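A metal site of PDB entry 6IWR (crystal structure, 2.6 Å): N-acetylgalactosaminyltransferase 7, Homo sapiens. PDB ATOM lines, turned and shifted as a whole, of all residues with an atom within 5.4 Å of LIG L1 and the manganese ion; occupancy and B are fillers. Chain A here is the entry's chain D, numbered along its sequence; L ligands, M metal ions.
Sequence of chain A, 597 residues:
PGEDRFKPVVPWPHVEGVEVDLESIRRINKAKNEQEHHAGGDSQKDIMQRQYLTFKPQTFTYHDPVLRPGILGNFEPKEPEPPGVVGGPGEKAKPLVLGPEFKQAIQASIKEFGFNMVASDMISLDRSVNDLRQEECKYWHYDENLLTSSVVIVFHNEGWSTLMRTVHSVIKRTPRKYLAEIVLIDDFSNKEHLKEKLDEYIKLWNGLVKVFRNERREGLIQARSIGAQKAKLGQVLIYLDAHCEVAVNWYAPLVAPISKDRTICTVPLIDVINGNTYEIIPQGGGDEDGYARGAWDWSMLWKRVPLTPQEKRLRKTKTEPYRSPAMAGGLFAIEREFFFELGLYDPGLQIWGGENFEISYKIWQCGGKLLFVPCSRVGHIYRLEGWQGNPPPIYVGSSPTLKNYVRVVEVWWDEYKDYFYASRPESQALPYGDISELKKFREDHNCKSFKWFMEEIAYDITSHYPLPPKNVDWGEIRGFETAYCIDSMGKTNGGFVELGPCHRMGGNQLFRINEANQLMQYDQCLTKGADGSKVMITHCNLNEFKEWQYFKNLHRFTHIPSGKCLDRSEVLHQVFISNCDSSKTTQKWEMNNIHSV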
ATOM      1  N   VAL A 154     -24.553  18.336  24.152  1.00  0.00           N
ATOM      2  CA  VAL A 154     -23.448  18.908  23.377  1.00  0.00           C
ATOM      3  C   VAL A 154     -22.900  20.135  24.092  1.00  0.00           C
ATOM      4  O   VAL A 154     -23.658  20.988  24.561  1.00  0.00           O
ATOM      5  CB  VAL A 154     -23.918  19.278  21.957  1.00  0.00           C
ATOM      6  CG1 VAL A 154     -22.796  19.996  21.191  1.00  0.00           C
ATOM      7  CG2 VAL A 154     -24.385  18.041  21.226  1.00  0.00           C
ATOM      8  N   PHE A 155     -21.571  20.236  24.164  1.00  0.00           N
ATOM      9  CA  PHE A 155     -20.959  21.347  24.870  1.00  0.00           C
ATOM     10  C   PHE A 155     -19.667  21.766  24.177  1.00  0.00           C
ATOM     11  O   PHE A 155     -18.920  20.932  23.660  1.00  0.00           O
ATOM     12  CB  PHE A 155     -20.677  20.997  26.337  1.00  0.00           C
ATOM     13  CG  PHE A 155     -19.591  19.978  26.536  1.00  0.00           C
ATOM     14  CD1 PHE A 155     -18.255  20.362  26.617  1.00  0.00           C
ATOM     15  CD2 PHE A 155     -19.893  18.633  26.695  1.00  0.00           C
ATOM     16  CE1 PHE A 155     -17.252  19.435  26.816  1.00  0.00           C
ATOM     17  CE2 PHE A 155     -18.892  17.695  26.913  1.00  0.00           C
ATOM     18  CZ  PHE A 155     -17.575  18.097  26.976  1.00  0.00           C
ATOM     19  N   HIS A 156     -19.421  23.078  24.177  1.00  0.00           N
ATOM     20  CA  HIS A 156     -18.212  23.665  23.605  1.00  0.00           C
ATOM     21  C   HIS A 156     -17.748  24.795  24.524  1.00  0.00           C
ATOM     22  O   HIS A 156     -18.401  25.835  24.595  1.00  0.00           O
ATOM     23  CB  HIS A 156     -18.451  24.199  22.190  1.00  0.00           C
ATOM     24  CG  HIS A 156     -17.208  24.720  21.541  1.00  0.00           C
ATOM     25  ND1 HIS A 156     -16.394  23.932  20.751  1.00  0.00           N
ATOM     26  CD2 HIS A 156     -16.621  25.940  21.584  1.00  0.00           C
ATOM     27  CE1 HIS A 156     -15.367  24.646  20.329  1.00  0.00           C
ATOM     28  NE2 HIS A 156     -15.489  25.870  20.813  1.00  0.00           N
ATOM     29  N   GLU A 158     -17.893  25.223  27.604  1.00  0.00           N
ATOM     30  CA  GLU A 158     -18.806  25.603  28.665  1.00  0.00           C
ATOM     31  C   GLU A 158     -18.097  25.721  30.008  1.00  0.00           C
ATOM     32  O   GLU A 158     -17.115  25.025  30.282  1.00  0.00           O
ATOM     33  CB  GLU A 158     -19.938  24.584  28.777  1.00  0.00           C
ATOM     34  CG  GLU A 158     -20.913  24.687  27.625  1.00  0.00           C
ATOM     35  CD  GLU A 158     -21.856  25.857  27.790  1.00  0.00           C
ATOM     36  OE1 GLU A 158     -22.223  26.466  26.752  1.00  0.00           O
ATOM     37  OE2 GLU A 158     -22.219  26.156  28.968  1.00  0.00           O
ATOM     38  N   ASP A 187     -17.533  18.908  21.685  1.00  0.00           N
ATOM     39  CA  ASP A 187     -17.256  19.363  20.324  1.00  0.00           C
ATOM     40  C   ASP A 187     -15.985  20.213  20.290  1.00  0.00           C
ATOM     41  O   ASP A 187     -15.980  21.373  19.889  1.00  0.00           O
ATOM     42  CB  ASP A 187     -18.447  20.132  19.762  1.00  0.00           C
ATOM     43  CG  ASP A 187     -18.336  20.334  18.274  1.00  0.00           C
ATOM     44  OD1 ASP A 187     -17.968  19.363  17.589  1.00  0.00           O
ATOM     45  OD2 ASP A 187     -18.635  21.449  17.791  1.00  0.00           O
ATOM     46  N   ARG A 217     -13.972  20.276  15.054  1.00  0.00           N
ATOM     47  CA  ARG A 217     -15.170  21.048  15.383  1.00  0.00           C
ATOM     48  C   ARG A 217     -16.254  20.724  14.373  1.00  0.00           C
ATOM     49  O   ARG A 217     -16.252  21.252  13.256  1.00  0.00           O
ATOM     50  CB  ARG A 217     -14.863  22.542  15.385  1.00  0.00           C
ATOM     51  CG  ARG A 217     -16.079  23.410  15.727  1.00  0.00           C
ATOM     52  CD  ARG A 217     -16.338  23.417  17.223  1.00  0.00           C
ATOM     53  NE  ARG A 217     -17.274  24.461  17.623  1.00  0.00           N
ATOM     54  CZ  ARG A 217     -16.934  25.739  17.834  1.00  0.00           C
ATOM     55  NH1 ARG A 217     -15.687  26.123  17.677  1.00  0.00           N
ATOM     56  NH2 ARG A 217     -17.854  26.626  18.202  1.00  0.00           N
ATOM     57  N   GLY A 219     -19.485  21.379  14.908  1.00  0.00           N
ATOM     58  CA  GLY A 219     -20.626  22.266  15.019  1.00  0.00           C
ATOM     59  C   GLY A 219     -21.816  21.592  15.689  1.00  0.00           C
ATOM     60  O   GLY A 219     -22.004  20.375  15.654  1.00  0.00           O
ATOM     61  N   LEU A 220     -22.623  22.426  16.352  1.00  0.00           N
ATOM     62  CA  LEU A 220     -23.639  21.883  17.252  1.00  0.00           C
ATOM     63  C   LEU A 220     -24.669  21.039  16.522  1.00  0.00           C
ATOM     64  O   LEU A 220     -25.150  20.037  17.068  1.00  0.00           O
ATOM     65  CB  LEU A 220     -24.322  23.008  18.022  1.00  0.00           C
ATOM     66  CG  LEU A 220     -25.079  24.023  17.168  1.00  0.00           C
ATOM     67  CD1 LEU A 220     -26.478  24.247  17.698  1.00  0.00           C
ATOM     68  CD2 LEU A 220     -24.301  25.355  17.037  1.00  0.00           C
ATOM     69  N   ALA A 223     -22.716  17.939  15.785  1.00  0.00           N
ATOM     70  CA  ALA A 223     -22.453  17.396  17.116  1.00  0.00           C
ATOM     71  C   ALA A 223     -23.665  16.641  17.645  1.00  0.00           C
ATOM     72  O   ALA A 223     -23.529  15.545  18.202  1.00  0.00           O
ATOM     73  CB  ALA A 223     -22.044  18.506  18.085  1.00  0.00           C
ATOM     74  N   ARG A 224     -24.859  17.218  17.484  1.00  0.00           N
ATOM     75  CA  ARG A 224     -26.075  16.551  17.947  1.00  0.00           C
ATOM     76  C   ARG A 224     -26.287  15.228  17.222  1.00  0.00           C
ATOM     77  O   ARG A 224     -26.760  14.251  17.823  1.00  0.00           O
ATOM     78  CB  ARG A 224     -27.278  17.464  17.735  1.00  0.00           C
ATOM     79  CG  ARG A 224     -27.475  18.474  18.834  1.00  0.00           C
ATOM     80  CD  ARG A 224     -28.897  18.985  18.833  1.00  0.00           C
ATOM     81  NE  ARG A 224     -28.963  20.315  19.411  1.00  0.00           N
ATOM     82  CZ  ARG A 224     -29.223  21.424  18.721  1.00  0.00           C
ATOM     83  NH1 ARG A 224     -29.465  21.361  17.421  1.00  0.00           N
ATOM     84  NH2 ARG A 224     -29.276  22.588  19.328  1.00  0.00           N
ATOM     85  N   LEU A 240     -30.333  18.384  25.395  1.00  0.00           N
ATOM     86  CA  LEU A 240     -30.250  19.508  26.321  1.00  0.00           C
ATOM     87  C   LEU A 240     -29.059  20.373  25.951  1.00  0.00           C
ATOM     88  O   LEU A 240     -28.042  19.893  25.443  1.00  0.00           O
ATOM     89  CB  LEU A 240     -30.103  19.067  27.781  1.00  0.00           C
ATOM     90  CG  LEU A 240     -31.280  18.966  28.777  1.00  0.00           C
ATOM     91  CD1 LEU A 240     -32.668  19.116  28.176  1.00  0.00           C
ATOM     92  CD2 LEU A 240     -31.209  17.662  29.593  1.00  0.00           C
ATOM     93  N   ASP A 241     -29.211  21.662  26.192  1.00  0.00           N
ATOM     94  CA  ASP A 241     -28.095  22.574  26.087  1.00  0.00           C
ATOM     95  C   ASP A 241     -27.195  22.388  27.305  1.00  0.00           C
ATOM     96  O   ASP A 241     -27.632  21.916  28.355  1.00  0.00           O
ATOM     97  CB  ASP A 241     -28.597  24.002  25.994  1.00  0.00           C
ATOM     98  CG  ASP A 241     -28.438  24.607  24.598  1.00  0.00           C
ATOM     99  OD1 ASP A 241     -28.632  23.887  23.610  1.00  0.00           O
ATOM    100  OD2 ASP A 241     -28.109  25.802  24.515  1.00  0.00           O
ATOM    101  N   ALA A 242     -25.914  22.731  27.154  1.00  0.00           N
ATOM    102  CA  ALA A 242     -24.953  22.598  28.239  1.00  0.00           C
ATOM    103  C   ALA A 242     -25.104  23.667  29.309  1.00  0.00           C
ATOM    104  O   ALA A 242     -24.165  23.923  30.068  1.00  0.00           O
ATOM    105  CB  ALA A 242     -23.549  22.607  27.680  1.00  0.00           C
ATOM    106  N   HIS A 243     -26.277  24.311  29.400  1.00  0.00           N
ATOM    107  CA  HIS A 243     -26.549  25.307  30.444  1.00  0.00           C
ATOM    108  C   HIS A 243     -28.053  25.332  30.648  1.00  0.00           C
ATOM    109  O   HIS A 243     -28.761  26.246  30.214  1.00  0.00           O
ATOM    110  CB  HIS A 243     -26.011  26.630  30.043  1.00  0.00           C
ATOM    111  CG  HIS A 243     -26.116  26.898  28.583  1.00  0.00           C
ATOM    112  ND1 HIS A 243     -25.063  26.728  27.719  1.00  0.00           N
ATOM    113  CD2 HIS A 243     -27.152  27.342  27.829  1.00  0.00           C
ATOM    114  CE1 HIS A 243     -25.434  27.068  26.498  1.00  0.00           C
ATOM    115  NE2 HIS A 243     -26.698  27.433  26.542  1.00  0.00           N
ATOM    116  N   ILE A 351     -22.577  25.246  10.958  1.00  0.00           N
ATOM    117  CA  ILE A 351     -22.441  25.317  12.378  1.00  0.00           C
ATOM    118  C   ILE A 351     -23.656  25.785  13.164  1.00  0.00           C
ATOM    119  O   ILE A 351     -23.994  25.157  14.147  1.00  0.00           O
ATOM    120  CB  ILE A 351     -21.279  26.236  12.760  1.00  0.00           C
ATOM    121  CG1 ILE A 351     -21.350  27.540  11.945  1.00  0.00           C
ATOM    122  CG2 ILE A 351     -19.965  25.487  12.634  1.00  0.00           C
ATOM    123  CD1 ILE A 351     -20.322  27.682  10.848  1.00  0.00           C
ATOM    124  N   TRP A 352     -24.325  26.850  12.758  1.00  0.00           N
ATOM    125  CA  TRP A 352     -25.493  27.311  13.505  1.00  0.00           C
ATOM    126  C   TRP A 352     -26.723  27.667  12.694  1.00  0.00           C
ATOM    127  O   TRP A 352     -26.670  28.470  11.783  1.00  0.00           O
ATOM    128  CB  TRP A 352     -25.100  28.488  14.410  1.00  0.00           C
ATOM    129  CG  TRP A 352     -26.184  28.918  15.348  1.00  0.00           C
ATOM    130  CD1 TRP A 352     -26.338  28.535  16.628  1.00  0.00           C
ATOM    131  CD2 TRP A 352     -27.257  29.811  15.062  1.00  0.00           C
ATOM    132  NE1 TRP A 352     -27.440  29.123  17.174  1.00  0.00           N
ATOM    133  CE2 TRP A 352     -28.017  29.919  16.224  1.00  0.00           C
ATOM    134  CE3 TRP A 352     -27.647  30.526  13.941  1.00  0.00           C
ATOM    135  CZ2 TRP A 352     -29.156  30.710  16.289  1.00  0.00           C
ATOM    136  CZ3 TRP A 352     -28.773  31.310  14.009  1.00  0.00           C
ATOM    137  CH2 TRP A 352     -29.512  31.397  15.172  1.00  0.00           C
ATOM    138  N   HIS A 380     -33.174  27.523  30.801  1.00  0.00           N
ATOM    139  CA  HIS A 380     -32.099  27.680  29.839  1.00  0.00           C
ATOM    140  C   HIS A 380     -31.377  28.985  30.176  1.00  0.00           C
ATOM    141  O   HIS A 380     -31.997  30.041  30.177  1.00  0.00           O
ATOM    142  CB  HIS A 380     -32.669  27.704  28.433  1.00  0.00           C
ATOM    143  CG  HIS A 380     -31.643  27.848  27.377  1.00  0.00           C
ATOM    144  ND1 HIS A 380     -31.423  29.029  26.711  1.00  0.00           N
ATOM    145  CD2 HIS A 380     -30.734  26.967  26.899  1.00  0.00           C
ATOM    146  CE1 HIS A 380     -30.436  28.872  25.847  1.00  0.00           C
ATOM    147  NE2 HIS A 380     -30.015  27.627  25.927  1.00  0.00           N
ATOM    148  N   ILE A 381     -30.090  28.894  30.549  1.00  0.00           N
ATOM    149  CA  ILE A 381     -29.325  30.117  30.766  1.00  0.00           C
ATOM    150  C   ILE A 381     -29.183  30.841  29.426  1.00  0.00           C
ATOM    151  O   ILE A 381     -28.986  30.217  28.373  1.00  0.00           O
ATOM    152  CB  ILE A 381     -27.938  29.875  31.379  1.00  0.00           C
ATOM    153  CG1 ILE A 381     -27.965  28.931  32.584  1.00  0.00           C
ATOM    154  CG2 ILE A 381     -27.336  31.194  31.833  1.00  0.00           C
ATOM    155  CD1 ILE A 381     -26.561  28.596  33.094  1.00  0.00           C
ATOM    156  N   ARG A 383     -27.398  33.945  27.098  1.00  0.00           N
ATOM    157  CA  ARG A 383     -26.067  34.526  27.049  1.00  0.00           C
ATOM    158  C   ARG A 383     -26.106  36.036  27.231  1.00  0.00           C
ATOM    159  O   ARG A 383     -26.933  36.717  26.625  1.00  0.00           O
ATOM    160  CB  ARG A 383     -25.398  34.154  25.732  1.00  0.00           C
ATOM    161  CG  ARG A 383     -25.812  32.761  25.219  1.00  0.00           C
ATOM    162  CD  ARG A 383     -24.761  32.156  24.312  1.00  0.00           C
ATOM    163  NE  ARG A 383     -23.561  31.756  25.051  1.00  0.00           N
ATOM    164  CZ  ARG A 383     -23.254  30.514  25.370  1.00  0.00           C
ATOM    165  NH1 ARG A 383     -24.068  29.516  25.023  1.00  0.00           N
ATOM    166  NH2 ARG A 383     -22.134  30.242  26.041  1.00  0.00           N
HETATM  167  N1  LIG L   1     -22.131  24.039  20.418  1.00  0.00           N
HETATM  168  C1  LIG L   1     -21.279  23.147  19.720  1.00  0.00           C
HETATM  169  N2  LIG L   1     -20.630  23.695  18.630  1.00  0.00           N
HETATM  170  C2  LIG L   1     -20.735  25.019  18.162  1.00  0.00           C
HETATM  171  C3  LIG L   1     -21.619  25.879  18.958  1.00  0.00           C
HETATM  172  C4  LIG L   1     -22.256  25.367  20.042  1.00  0.00           C
HETATM  173  O1  LIG L   1     -21.142  21.950  20.030  1.00  0.00           O
HETATM  174  O2  LIG L   1     -20.073  25.384  17.130  1.00  0.00           O
HETATM  175  C5  LIG L   1     -22.809  23.496  21.604  1.00  0.00           C
HETATM  176  C6  LIG L   1     -22.939  24.489  22.794  1.00  0.00           C
HETATM  177  O3  LIG L   1     -21.990  24.203  23.836  1.00  0.00           O
HETATM  178  C7  LIG L   1     -24.427  24.310  23.238  1.00  0.00           C
HETATM  179  C8  LIG L   1     -25.107  23.919  21.931  1.00  0.00           C
HETATM  180  O4  LIG L   1     -24.124  23.140  21.205  1.00  0.00           O
HETATM  181  O5  LIG L   1     -24.601  23.325  24.293  1.00  0.00           O
HETATM  182  C9  LIG L   1     -25.593  25.073  21.099  1.00  0.00           C
HETATM  183  O6  LIG L   1     -26.255  26.031  21.959  1.00  0.00           O
HETATM  184  P1  LIG L   1     -25.952  27.615  21.871  1.00  0.00           P
HETATM  185  O7  LIG L   1     -24.591  27.908  21.159  1.00  0.00           O
HETATM  186  O8  LIG L   1     -26.075  28.151  23.262  1.00  0.00           O
HETATM  187  O9  LIG L   1     -27.215  28.254  20.861  1.00  0.00           O
HETATM  188  P2  LIG L   1     -28.296  29.149  21.639  1.00  0.00           P
HETATM  189  O10 LIG L   1     -29.240  29.933  20.633  1.00  0.00           O
HETATM  190  O11 LIG L   1     -27.374  30.091  22.649  1.00  0.00           O
HETATM  191  O12 LIG L   1     -29.140  28.108  22.385  1.00  0.00           O
HETATM  192  C1  LG2 L   2     -31.933  28.089  19.526  1.00  0.00           C
HETATM  193  C2  LG2 L   2     -31.651  26.796  20.334  1.00  0.00           C
HETATM  194  C3  LG2 L   2     -30.305  26.176  19.853  1.00  0.00           C
HETATM  195  C4  LG2 L   2     -30.393  25.871  18.344  1.00  0.00           C
HETATM  196  C5  LG2 L   2     -30.799  27.164  17.578  1.00  0.00           C
HETATM  197  C6  LG2 L   2     -30.912  26.925  16.077  1.00  0.00           C
HETATM  198  C7  LG2 L   2     -32.760  26.944  22.502  1.00  0.00           C
HETATM  199  C8  LG2 L   2     -32.593  27.391  23.922  1.00  0.00           C
HETATM  200  N1  LG2 L   2     -31.654  27.074  21.758  1.00  0.00           N
HETATM  201  O1  LG2 L   2     -33.012  28.814  20.071  1.00  0.00           O
HETATM  202  O2  LG2 L   2     -29.903  24.998  20.612  1.00  0.00           O
HETATM  203  O3  LG2 L   2     -29.112  25.423  17.860  1.00  0.00           O
HETATM  204  O4  LG2 L   2     -32.062  27.729  18.035  1.00  0.00           O
HETATM  205  O5  LG2 L   2     -29.631  26.720  15.443  1.00  0.00           O
HETATM  206  O6  LG2 L   2     -33.821  26.423  22.077  1.00  0.00           O
HETATM  207 MN    MN M   1     -28.067  27.811  24.554  1.00  0.00          MN
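The nearest printed residue that does not touch the manganese ion is Arg 383 (4.4 Å).
An oxygen (O12) of LIG L1 sits close to a nitrogen (N1) of LG2 L2, 2.8 Å away.
The backbone carbonyl oxygen (O) of Val 154 lies within hydrogen-bond range of an oxygen (O5) of LIG L1 (2.5 Å). O2 of LIG L1 lies within hydrogen-bond range of NH2 of Arg 217, at 2.8 Å. An oxygen (O3) of LIG L1 sits at hydrogen-bond distance from the backbone NH of His 156 (2.8 Å). NH1 of Arg 383 sits close to O8 of LIG L1 (3.0 Å). An oxygen (O2) of LG2 L2 is in hydrogen-bond range of the side-chain carboxylate of Asp 241, at 3.4 Å. O2 of LG2 L2 is in hydrogen-bond range of NH2 of Arg 224, at 2.8 Å. An oxygen (O5) of LIG L1 sits at hydrogen-bond distance from the backbone NH of Ala 242, at 3.2 Å. A nitrogen (N2) of LIG L1 is in hydrogen-bond range of the side-chain carboxylate of Asp 187 (3.1 Å).
N2 of LIG L1 sits close to N of Leu 220 (3.3 Å). Merely in contact with LIG L1: Phe 155, Glu 158, Gly 219 and Trp 352. Hydrophobic or aromatic side chains within 4 Å of LIG L1: Val 154, His 156, Leu 220, Ala 242, His 243 and His 380. Within 4 Å of LIG L1: Val 154, Phe 155, His 156, Glu 158, Asp 187, Arg 217, Gly 219, Leu 220, Asp 241, Ala 242, His 243, Trp 352, His 380 and Arg 383. Along chain A the residues within 4 Å of LIG L1 span positions 154 to 383. The nearest printed residue that does not touch LIG L1 is Ala 223 (4.1 Å).
The manganese ion is bound by the side-chain carboxylate (OD2) of Asp 241 (2.0 Å), a ring nitrogen (NE2) of His 380 (2.4 Å), an oxygen (O8) of LIG L1 (2.4 Å), an oxygen (O12) of LIG L1 (2.4 Å) and a ring nitrogen (NE2) of His 243 (2.4 Å).
The side-chain carboxylate of Glu 158 is in salt-bridge range of the guanidinium group of Arg 383 (3.8 Å). The guanidinium group (NH1) of Arg 217 lies close to a ring nitrogen (NE2) of His 156 (3.2 Å). N of Asp 187 lies within hydrogen-bond range of O of Phe 155, 3.1 Å away. O of His 243 sits at hydrogen-bond distance from N of Ile 381, at 3.0 Å. OE1 of Glu 158 sits at hydrogen-bond distance from ND1 of His 243 (3.0 Å). The side-chain carboxylate (OD2) of Asp 187 is in hydrogen-bond range of the backbone NH (N) of Gly 219, at 3.0 Å. A ring nitrogen (ND1) of His 156 is in hydrogen-bond range of the backbone carbonyl oxygen (O) of Asp 187 (2.7 Å). NE of Arg 217 lies within salt-bridge range of OD2 of Asp 187, at 3.3 Å.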
